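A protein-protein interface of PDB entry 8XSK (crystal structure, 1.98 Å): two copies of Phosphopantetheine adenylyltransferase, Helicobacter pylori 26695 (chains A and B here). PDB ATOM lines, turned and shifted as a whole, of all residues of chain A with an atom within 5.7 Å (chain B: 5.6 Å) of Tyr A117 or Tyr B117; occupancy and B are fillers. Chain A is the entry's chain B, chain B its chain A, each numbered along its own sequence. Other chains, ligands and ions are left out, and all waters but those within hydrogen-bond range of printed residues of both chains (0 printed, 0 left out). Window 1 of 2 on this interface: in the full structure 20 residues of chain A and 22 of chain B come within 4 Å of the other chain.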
ATOM      1  N   LEU A  86       7.155  -0.891  21.519  1.00  0.00           N
ATOM      2  CA  LEU A  86       8.343  -1.328  22.307  1.00  0.00           C
ATOM      3  C   LEU A  86       8.413  -2.851  22.330  1.00  0.00           C
ATOM      4  O   LEU A  86       7.404  -3.493  22.700  1.00  0.00           O
ATOM      5  CB  LEU A  86       8.242  -0.737  23.720  1.00  0.00           C
ATOM      6  CG  LEU A  86       8.348   0.786  23.786  1.00  0.00           C
ATOM      7  CD1 LEU A  86       8.296   1.295  25.232  1.00  0.00           C
ATOM      8  CD2 LEU A  86       9.607   1.274  23.103  1.00  0.00           C
ATOM      9  N   ARG A  88      10.013  -6.085  24.077  1.00  0.00           N
ATOM     10  CA  ARG A  88      10.595  -6.508  25.373  1.00  0.00           C
ATOM     11  C   ARG A  88      10.683  -8.026  25.335  1.00  0.00           C
ATOM     12  O   ARG A  88       9.951  -8.658  24.508  1.00  0.00           O
ATOM     13  CB  ARG A  88       9.723  -6.062  26.561  1.00  0.00           C
ATOM     14  CG  ARG A  88       9.678  -4.573  26.851  1.00  0.00           C
ATOM     15  CD  ARG A  88      11.031  -3.955  27.157  1.00  0.00           C
ATOM     16  NE  ARG A  88      11.084  -2.672  27.888  1.00  0.00           N
ATOM     17  CZ  ARG A  88      10.084  -1.804  28.081  1.00  0.00           C
ATOM     18  NH1 ARG A  88      10.316  -0.690  28.752  1.00  0.00           N
ATOM     19  NH2 ARG A  88       8.862  -2.018  27.617  1.00  0.00           N
ATOM     20  N   GLY A  89      11.571  -8.584  26.157  1.00  0.00           N
ATOM     21  CA  GLY A  89      11.901 -10.028  26.176  1.00  0.00           C
ATOM     22  C   GLY A  89      11.477 -10.591  27.513  1.00  0.00           C
ATOM     23  O   GLY A  89      11.551  -9.809  28.468  1.00  0.00           O
ATOM     24  N   LEU A  90      10.885 -11.792  27.555  1.00  0.00           N
ATOM     25  CA  LEU A  90      10.393 -12.439  28.798  1.00  0.00           C
ATOM     26  C   LEU A  90      11.190 -13.718  29.021  1.00  0.00           C
ATOM     27  O   LEU A  90      11.406 -14.450  28.043  1.00  0.00           O
ATOM     28  CB  LEU A  90       8.915 -12.817  28.664  1.00  0.00           C
ATOM     29  CG  LEU A  90       7.927 -11.668  28.726  1.00  0.00           C
ATOM     30  CD1 LEU A  90       6.522 -12.207  28.822  1.00  0.00           C
ATOM     31  CD2 LEU A  90       8.218 -10.717  29.871  1.00  0.00           C
ATOM     32  N   GLU A  99       7.204  -5.751  34.431  1.00  0.00           N
ATOM     33  CA  GLU A  99       7.123  -5.558  32.945  1.00  0.00           C
ATOM     34  C   GLU A  99       5.787  -4.939  32.530  1.00  0.00           C
ATOM     35  O   GLU A  99       5.797  -4.006  31.671  1.00  0.00           O
ATOM     36  CB  GLU A  99       7.346  -6.874  32.209  1.00  0.00           C
ATOM     37  CG  GLU A  99       8.777  -7.336  32.305  1.00  0.00           C
ATOM     38  CD  GLU A  99       9.732  -6.531  31.418  1.00  0.00           C
ATOM     39  OE1 GLU A  99       9.276  -5.949  30.404  1.00  0.00           O
ATOM     40  OE2 GLU A  99      10.897  -6.417  31.789  1.00  0.00           O
ATOM     41  N   LEU A 100       4.669  -5.411  33.091  1.00  0.00           N
ATOM     42  CA  LEU A 100       3.340  -4.845  32.756  1.00  0.00           C
ATOM     43  C   LEU A 100       3.288  -3.364  33.159  1.00  0.00           C
ATOM     44  O   LEU A 100       2.724  -2.575  32.392  1.00  0.00           O
ATOM     45  CB  LEU A 100       2.243  -5.598  33.494  1.00  0.00           C
ATOM     46  CG  LEU A 100       2.059  -7.054  33.123  1.00  0.00           C
ATOM     47  CD1 LEU A 100       0.897  -7.617  33.904  1.00  0.00           C
ATOM     48  CD2 LEU A 100       1.825  -7.221  31.627  1.00  0.00           C
ATOM     49  N   MET A 102       5.645  -1.161  33.476  1.00  0.00           N
ATOM     50  CA  MET A 102       6.462  -0.384  32.508  1.00  0.00           C
ATOM     51  C   MET A 102       5.688  -0.237  31.197  1.00  0.00           C
ATOM     52  O   MET A 102       5.743   0.841  30.626  1.00  0.00           O
ATOM     53  CB  MET A 102       7.795  -1.063  32.204  1.00  0.00           C
ATOM     54  CG  MET A 102       8.932  -0.095  31.951  1.00  0.00           C
ATOM     55  SD  MET A 102      10.515  -0.816  32.498  1.00  0.00           S
ATOM     56  CE  MET A 102      10.451  -2.418  31.680  1.00  0.00           C
ATOM     57  N   GLY A 103       4.995  -1.283  30.760  1.00  0.00           N
ATOM     58  CA  GLY A 103       4.173  -1.221  29.538  1.00  0.00           C
ATOM     59  C   GLY A 103       3.084  -0.163  29.650  1.00  0.00           C
ATOM     60  O   GLY A 103       3.021   0.759  28.782  1.00  0.00           O
ATOM     61  N   THR A 115       3.428  -2.319  23.966  1.00  0.00           N
ATOM     62  CA  THR A 115       4.578  -3.196  24.287  1.00  0.00           C
ATOM     63  C   THR A 115       4.242  -4.630  23.898  1.00  0.00           C
ATOM     64  O   THR A 115       3.153  -5.128  24.275  1.00  0.00           O
ATOM     65  CB  THR A 115       4.984  -3.165  25.764  1.00  0.00           C
ATOM     66  OG1 THR A 115       5.185  -1.802  26.124  1.00  0.00           O
ATOM     67  CG2 THR A 115       6.254  -3.979  26.006  1.00  0.00           C
ATOM     68  N   LEU A 116       5.160  -5.254  23.175  1.00  0.00           N
ATOM     69  CA  LEU A 116       5.081  -6.644  22.679  1.00  0.00           C
ATOM     70  C   LEU A 116       6.249  -7.466  23.238  1.00  0.00           C
ATOM     71  O   LEU A 116       7.428  -7.067  23.062  1.00  0.00           O
ATOM     72  CB  LEU A 116       5.188  -6.543  21.160  1.00  0.00           C
ATOM     73  CG  LEU A 116       5.040  -7.827  20.373  1.00  0.00           C
ATOM     74  CD1 LEU A 116       3.730  -8.505  20.730  1.00  0.00           C
ATOM     75  CD2 LEU A 116       5.128  -7.522  18.888  1.00  0.00           C
ATOM     76  N   TYR A 117       5.931  -8.624  23.773  1.00  0.00           N
ATOM     77  CA  TYR A 117       6.889  -9.518  24.474  1.00  0.00           C
ATOM     78  C   TYR A 117       7.196 -10.773  23.667  1.00  0.00           C
ATOM     79  O   TYR A 117       6.254 -11.523  23.243  1.00  0.00           O
ATOM     80  CB  TYR A 117       6.316  -9.933  25.819  1.00  0.00           C
ATOM     81  CG  TYR A 117       5.971  -8.757  26.679  1.00  0.00           C
ATOM     82  CD1 TYR A 117       4.767  -8.080  26.540  1.00  0.00           C
ATOM     83  CD2 TYR A 117       6.894  -8.261  27.578  1.00  0.00           C
ATOM     84  CE1 TYR A 117       4.473  -6.968  27.308  1.00  0.00           C
ATOM     85  CE2 TYR A 117       6.621  -7.146  28.340  1.00  0.00           C
ATOM     86  CZ  TYR A 117       5.406  -6.510  28.221  1.00  0.00           C
ATOM     87  OH  TYR A 117       5.157  -5.439  29.013  1.00  0.00           O
ATOM     88  N   PHE A 118       8.491 -11.025  23.520  1.00  0.00           N
ATOM     89  CA  PHE A 118       9.049 -12.232  22.872  1.00  0.00           C
ATOM     90  C   PHE A 118       9.714 -13.115  23.930  1.00  0.00           C
ATOM     91  O   PHE A 118      10.054 -12.653  25.047  1.00  0.00           O
ATOM     92  CB  PHE A 118      10.021 -11.859  21.754  1.00  0.00           C
ATOM     93  CG  PHE A 118       9.424 -11.053  20.630  1.00  0.00           C
ATOM     94  CD1 PHE A 118       8.938  -9.777  20.843  1.00  0.00           C
ATOM     95  CD2 PHE A 118       9.329 -11.593  19.359  1.00  0.00           C
ATOM     96  CE1 PHE A 118       8.430  -9.027  19.792  1.00  0.00           C
ATOM     97  CE2 PHE A 118       8.793 -10.859  18.324  1.00  0.00           C
ATOM     98  CZ  PHE A 118       8.332  -9.585  18.547  1.00  0.00           C
ATOM     99  N   MET A 119       9.865 -14.380  23.566  1.00  0.00           N
ATOM    100  CA  MET A 119      10.566 -15.405  24.368  1.00  0.00           C
ATOM    101  C   MET A 119      11.869 -15.685  23.652  1.00  0.00           C
ATOM    102  O   MET A 119      11.869 -15.743  22.427  1.00  0.00           O
ATOM    103  CB  MET A 119       9.774 -16.713  24.429  1.00  0.00           C
ATOM    104  CG  MET A 119       8.314 -16.518  24.678  1.00  0.00           C
ATOM    105  SD  MET A 119       7.366 -18.067  24.690  1.00  0.00           S
ATOM    106  CE  MET A 119       8.471 -19.190  25.533  1.00  0.00           C
ATOM    107  N   LEU B  86       2.134 -17.835  17.357  1.00  0.00           N
ATOM    108  CA  LEU B  86       0.970 -17.855  18.281  1.00  0.00           C
ATOM    109  C   LEU B  86       0.927 -16.530  19.048  1.00  0.00           C
ATOM    110  O   LEU B  86       1.996 -15.997  19.416  1.00  0.00           O
ATOM    111  CB  LEU B  86       1.089 -19.048  19.236  1.00  0.00           C
ATOM    112  CG  LEU B  86       1.054 -20.430  18.581  1.00  0.00           C
ATOM    113  CD1 LEU B  86       1.234 -21.517  19.649  1.00  0.00           C
ATOM    114  CD2 LEU B  86      -0.275 -20.622  17.847  1.00  0.00           C
ATOM    115  N   ARG B  88      -0.600 -14.620  22.357  1.00  0.00           N
ATOM    116  CA  ARG B  88      -1.258 -14.767  23.669  1.00  0.00           C
ATOM    117  C   ARG B  88      -1.294 -13.392  24.326  1.00  0.00           C
ATOM    118  O   ARG B  88      -0.514 -12.484  23.912  1.00  0.00           O
ATOM    119  CB  ARG B  88      -0.557 -15.825  24.529  1.00  0.00           C
ATOM    120  CG  ARG B  88      -0.293 -17.172  23.859  1.00  0.00           C
ATOM    121  CD  ARG B  88      -1.248 -18.305  24.180  1.00  0.00           C
ATOM    122  NE  ARG B  88      -1.533 -18.414  25.618  1.00  0.00           N
ATOM    123  CZ  ARG B  88      -2.740 -18.685  26.143  1.00  0.00           C
ATOM    124  NH1 ARG B  88      -3.782 -18.891  25.348  1.00  0.00           N
ATOM    125  NH2 ARG B  88      -2.902 -18.767  27.460  1.00  0.00           N
ATOM    126  N   GLY B  89      -2.198 -13.232  25.284  1.00  0.00           N
ATOM    127  CA  GLY B  89      -2.279 -12.024  26.115  1.00  0.00           C
ATOM    128  C   GLY B  89      -1.654 -12.222  27.477  1.00  0.00           C
ATOM    129  O   GLY B  89      -1.624 -13.339  27.952  1.00  0.00           O
ATOM    130  N   LEU B  90      -1.162 -11.149  28.079  1.00  0.00           N
ATOM    131  CA  LEU B  90      -0.613 -11.177  29.447  1.00  0.00           C
ATOM    132  C   LEU B  90      -1.362 -10.169  30.317  1.00  0.00           C
ATOM    133  O   LEU B  90      -1.431  -8.980  29.926  1.00  0.00           O
ATOM    134  CB  LEU B  90       0.873 -10.843  29.406  1.00  0.00           C
ATOM    135  CG  LEU B  90       1.791 -11.872  28.784  1.00  0.00           C
ATOM    136  CD1 LEU B  90       3.215 -11.364  28.908  1.00  0.00           C
ATOM    137  CD2 LEU B  90       1.645 -13.252  29.429  1.00  0.00           C
ATOM    138  N   GLU B  99       2.571 -19.777  31.038  1.00  0.00           N
ATOM    139  CA  GLU B  99       2.520 -19.250  29.652  1.00  0.00           C
ATOM    140  C   GLU B  99       3.820 -19.606  28.941  1.00  0.00           C
ATOM    141  O   GLU B  99       3.740 -20.099  27.795  1.00  0.00           O
ATOM    142  CB  GLU B  99       2.347 -17.734  29.607  1.00  0.00           C
ATOM    143  CG  GLU B  99       1.013 -17.274  30.157  1.00  0.00           C
ATOM    144  CD  GLU B  99      -0.171 -17.614  29.276  1.00  0.00           C
ATOM    145  OE1 GLU B  99      -0.027 -17.557  28.016  1.00  0.00           O
ATOM    146  OE2 GLU B  99      -1.217 -17.977  29.840  1.00  0.00           O
ATOM    147  N   LEU B 100       4.956 -19.282  29.577  1.00  0.00           N
ATOM    148  CA  LEU B 100       6.304 -19.746  29.152  1.00  0.00           C
ATOM    149  C   LEU B 100       6.266 -21.244  28.817  1.00  0.00           C
ATOM    150  O   LEU B 100       6.528 -21.610  27.676  1.00  0.00           O
ATOM    151  CB  LEU B 100       7.312 -19.428  30.266  1.00  0.00           C
ATOM    152  CG  LEU B 100       7.663 -17.947  30.413  1.00  0.00           C
ATOM    153  CD1 LEU B 100       8.987 -17.792  31.128  1.00  0.00           C
ATOM    154  CD2 LEU B 100       7.729 -17.249  29.063  1.00  0.00           C
ATOM    155  N   GLY B 103       4.257 -21.992  25.719  1.00  0.00           N
ATOM    156  CA  GLY B 103       5.150 -21.530  24.634  1.00  0.00           C
ATOM    157  C   GLY B 103       6.183 -22.583  24.263  1.00  0.00           C
ATOM    158  O   GLY B 103       6.273 -22.959  23.061  1.00  0.00           O
ATOM    159  N   THR B 115       5.797 -18.005  20.163  1.00  0.00           N
ATOM    160  CA  THR B 115       4.725 -17.302  20.901  1.00  0.00           C
ATOM    161  C   THR B 115       5.119 -15.850  21.189  1.00  0.00           C
ATOM    162  O   THR B 115       6.262 -15.567  21.582  1.00  0.00           O
ATOM    163  CB  THR B 115       4.354 -17.983  22.219  1.00  0.00           C
ATOM    164  OG1 THR B 115       3.878 -19.303  21.956  1.00  0.00           O
ATOM    165  CG2 THR B 115       3.269 -17.216  22.958  1.00  0.00           C
ATOM    166  N   LEU B 116       4.168 -14.968  20.917  1.00  0.00           N
ATOM    167  CA  LEU B 116       4.267 -13.515  21.036  1.00  0.00           C
ATOM    168  C   LEU B 116       3.205 -13.075  22.033  1.00  0.00           C
ATOM    169  O   LEU B 116       2.068 -13.506  21.847  1.00  0.00           O
ATOM    170  CB  LEU B 116       3.998 -12.968  19.636  1.00  0.00           C
ATOM    171  CG  LEU B 116       4.205 -11.483  19.482  1.00  0.00           C
ATOM    172  CD1 LEU B 116       5.472 -11.081  20.227  1.00  0.00           C
ATOM    173  CD2 LEU B 116       4.307 -11.126  18.007  1.00  0.00           C
ATOM    174  N   TYR B 117       3.551 -12.226  22.996  1.00  0.00           N
ATOM    175  CA  TYR B 117       2.620 -11.734  24.042  1.00  0.00           C
ATOM    176  C   TYR B 117       2.291 -10.242  23.915  1.00  0.00           C
ATOM    177  O   TYR B 117       3.182  -9.343  23.902  1.00  0.00           O
ATOM    178  CB  TYR B 117       3.181 -12.030  25.430  1.00  0.00           C
ATOM    179  CG  TYR B 117       3.457 -13.487  25.694  1.00  0.00           C
ATOM    180  CD1 TYR B 117       2.452 -14.358  26.060  1.00  0.00           C
ATOM    181  CD2 TYR B 117       4.735 -13.997  25.556  1.00  0.00           C
ATOM    182  CE1 TYR B 117       2.706 -15.706  26.287  1.00  0.00           C
ATOM    183  CE2 TYR B 117       5.013 -15.328  25.800  1.00  0.00           C
ATOM    184  CZ  TYR B 117       3.996 -16.186  26.164  1.00  0.00           C
ATOM    185  OH  TYR B 117       4.271 -17.503  26.373  1.00  0.00           O
ATOM    186  N   PHE B 118       0.989  -9.969  23.960  1.00  0.00           N
ATOM    187  CA  PHE B 118       0.416  -8.610  23.888  1.00  0.00           C
ATOM    188  C   PHE B 118      -0.177  -8.331  25.273  1.00  0.00           C
ATOM    189  O   PHE B 118      -0.380  -9.279  26.071  1.00  0.00           O
ATOM    190  CB  PHE B 118      -0.575  -8.509  22.713  1.00  0.00           C
ATOM    191  CG  PHE B 118       0.011  -8.536  21.319  1.00  0.00           C
ATOM    192  CD1 PHE B 118       0.367  -9.731  20.703  1.00  0.00           C
ATOM    193  CD2 PHE B 118       0.131  -7.369  20.570  1.00  0.00           C
ATOM    194  CE1 PHE B 118       0.867  -9.759  19.407  1.00  0.00           C
ATOM    195  CE2 PHE B 118       0.628  -7.402  19.275  1.00  0.00           C
ATOM    196  CZ  PHE B 118       0.990  -8.601  18.686  1.00  0.00           C
ATOM    197  N   MET B 119      -0.456  -7.072  25.567  1.00  0.00           N
ATOM    198  CA  MET B 119      -1.164  -6.666  26.817  1.00  0.00           C
ATOM    199  C   MET B 119      -2.511  -6.089  26.423  1.00  0.00           C
ATOM    200  O   MET B 119      -2.584  -5.325  25.442  1.00  0.00           O
ATOM    201  CB  MET B 119      -0.393  -5.576  27.564  1.00  0.00           C
ATOM    202  CG  MET B 119       1.076  -5.916  27.834  1.00  0.00           C
ATOM    203  SD  MET B 119       1.947  -4.352  28.223  1.00  0.00           S
ATOM    204  CE  MET B 119       1.007  -3.794  29.632  1.00  0.00           C
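The backbone carbonyl oxygen of Tyr A117 sits at hydrogen-bond distance from the backbone NH of Tyr B117.
The side-chain sulfur (SD) of Met A119 sits at hydrogen-bond distance from the side-chain hydroxyl (OH) of Tyr B117 (3.6 Å).
The side-chain sulfur (SD) of Met B119 sits at hydrogen-bond distance from the side-chain hydroxyl (OH) of Tyr A117 (3.5 Å).
The backbone carbonyl oxygen of Arg B88 is in hydrogen-bond range of the backbone NH of Phe B118, at 2.9 Å.
The backbone NH (N) of Leu B90 lies within hydrogen-bond range of the backbone carbonyl oxygen (O) of Phe B118, at 2.9 Å.
OH of Tyr B117 sits at hydrogen-bond distance from O of Glu B99 (3.0 Å).
The backbone NH of Leu A116 is in hydrogen-bond range of the backbone carbonyl oxygen of Leu A86.
N of Arg A88 lies within hydrogen-bond range of O of Leu A116 (2.9 Å).
The side-chain hydroxyl of Tyr A117 is in hydrogen-bond range of the backbone carbonyl oxygen of Glu A99 (3.1 Å).
Among the printed residues, pairs that only touch across the chains: Leu A90 with Leu B90 (3.4 Å), Leu A100 with Met B119 (3.5 Å), Leu A116 with Leu B116 (3.2 Å), Leu A116 with Tyr B117 (3.3 Å), Leu A116 with Phe B118 (3.4 Å), Tyr A117 with Leu B116 (3.1 Å), Phe A118 with Leu B116 (3.6 Å), Met A119 with Leu B100 (3.8 Å) and Met A119 with Thr B115 (3.8 Å).
Of chain A, only Leu A116, Tyr A117 and Met A119 come within 4 Å of Tyr B117.
Of the printed residues of chain B, Phe A118 touches Leu B116.
Of the printed residues of chain B, Leu A116 touches Leu B116 (3.2 Å), Tyr B117 (3.3 Å) and Phe B118 (3.4 Å).
Of the printed residues of chain A, Met B119 touches Leu A100 and Tyr A117.
Arg B88 touches none of the printed residues of chain A.
The nearest residue of chain B that does not touch Tyr A117 is Leu B90 (4.3 Å).
The nearest residue of chain A that does not touch Tyr B117 is Leu A90 (4.1 Å).
Hydrophobic or aromatic side chains of chain B within 4 Å of the printed part of chain A: Leu B90, Leu B116, Tyr B117, Phe B118 and Met B119.
Of the 13 printed residues of chain A, 6 touch a printed residue of chain B.
Hydrophobic or aromatic side chains of chain A that line the printed part of chain B: Leu A90, Leu A116, Tyr A117, Phe A118 and Met A119.
Among the printed residues, no Asp or Glu carboxylate lies within 4 Å of a Lys or Arg side-chain nitrogen of the other chain.
Leu B90 touches its own counterpart, Leu A90.
Leu A100 touches Met B119, and with the chains exchanged Met A119 touches Leu B100.
Leu A116 touches its own counterpart, Leu B116.
Tyr B117 touches its own counterpart, Tyr A117.
12 positions are printed for both chains.
Of the 12 pairs that touch across the chains among the printed residues, 11 have their exchanged pair printed and touching as well.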
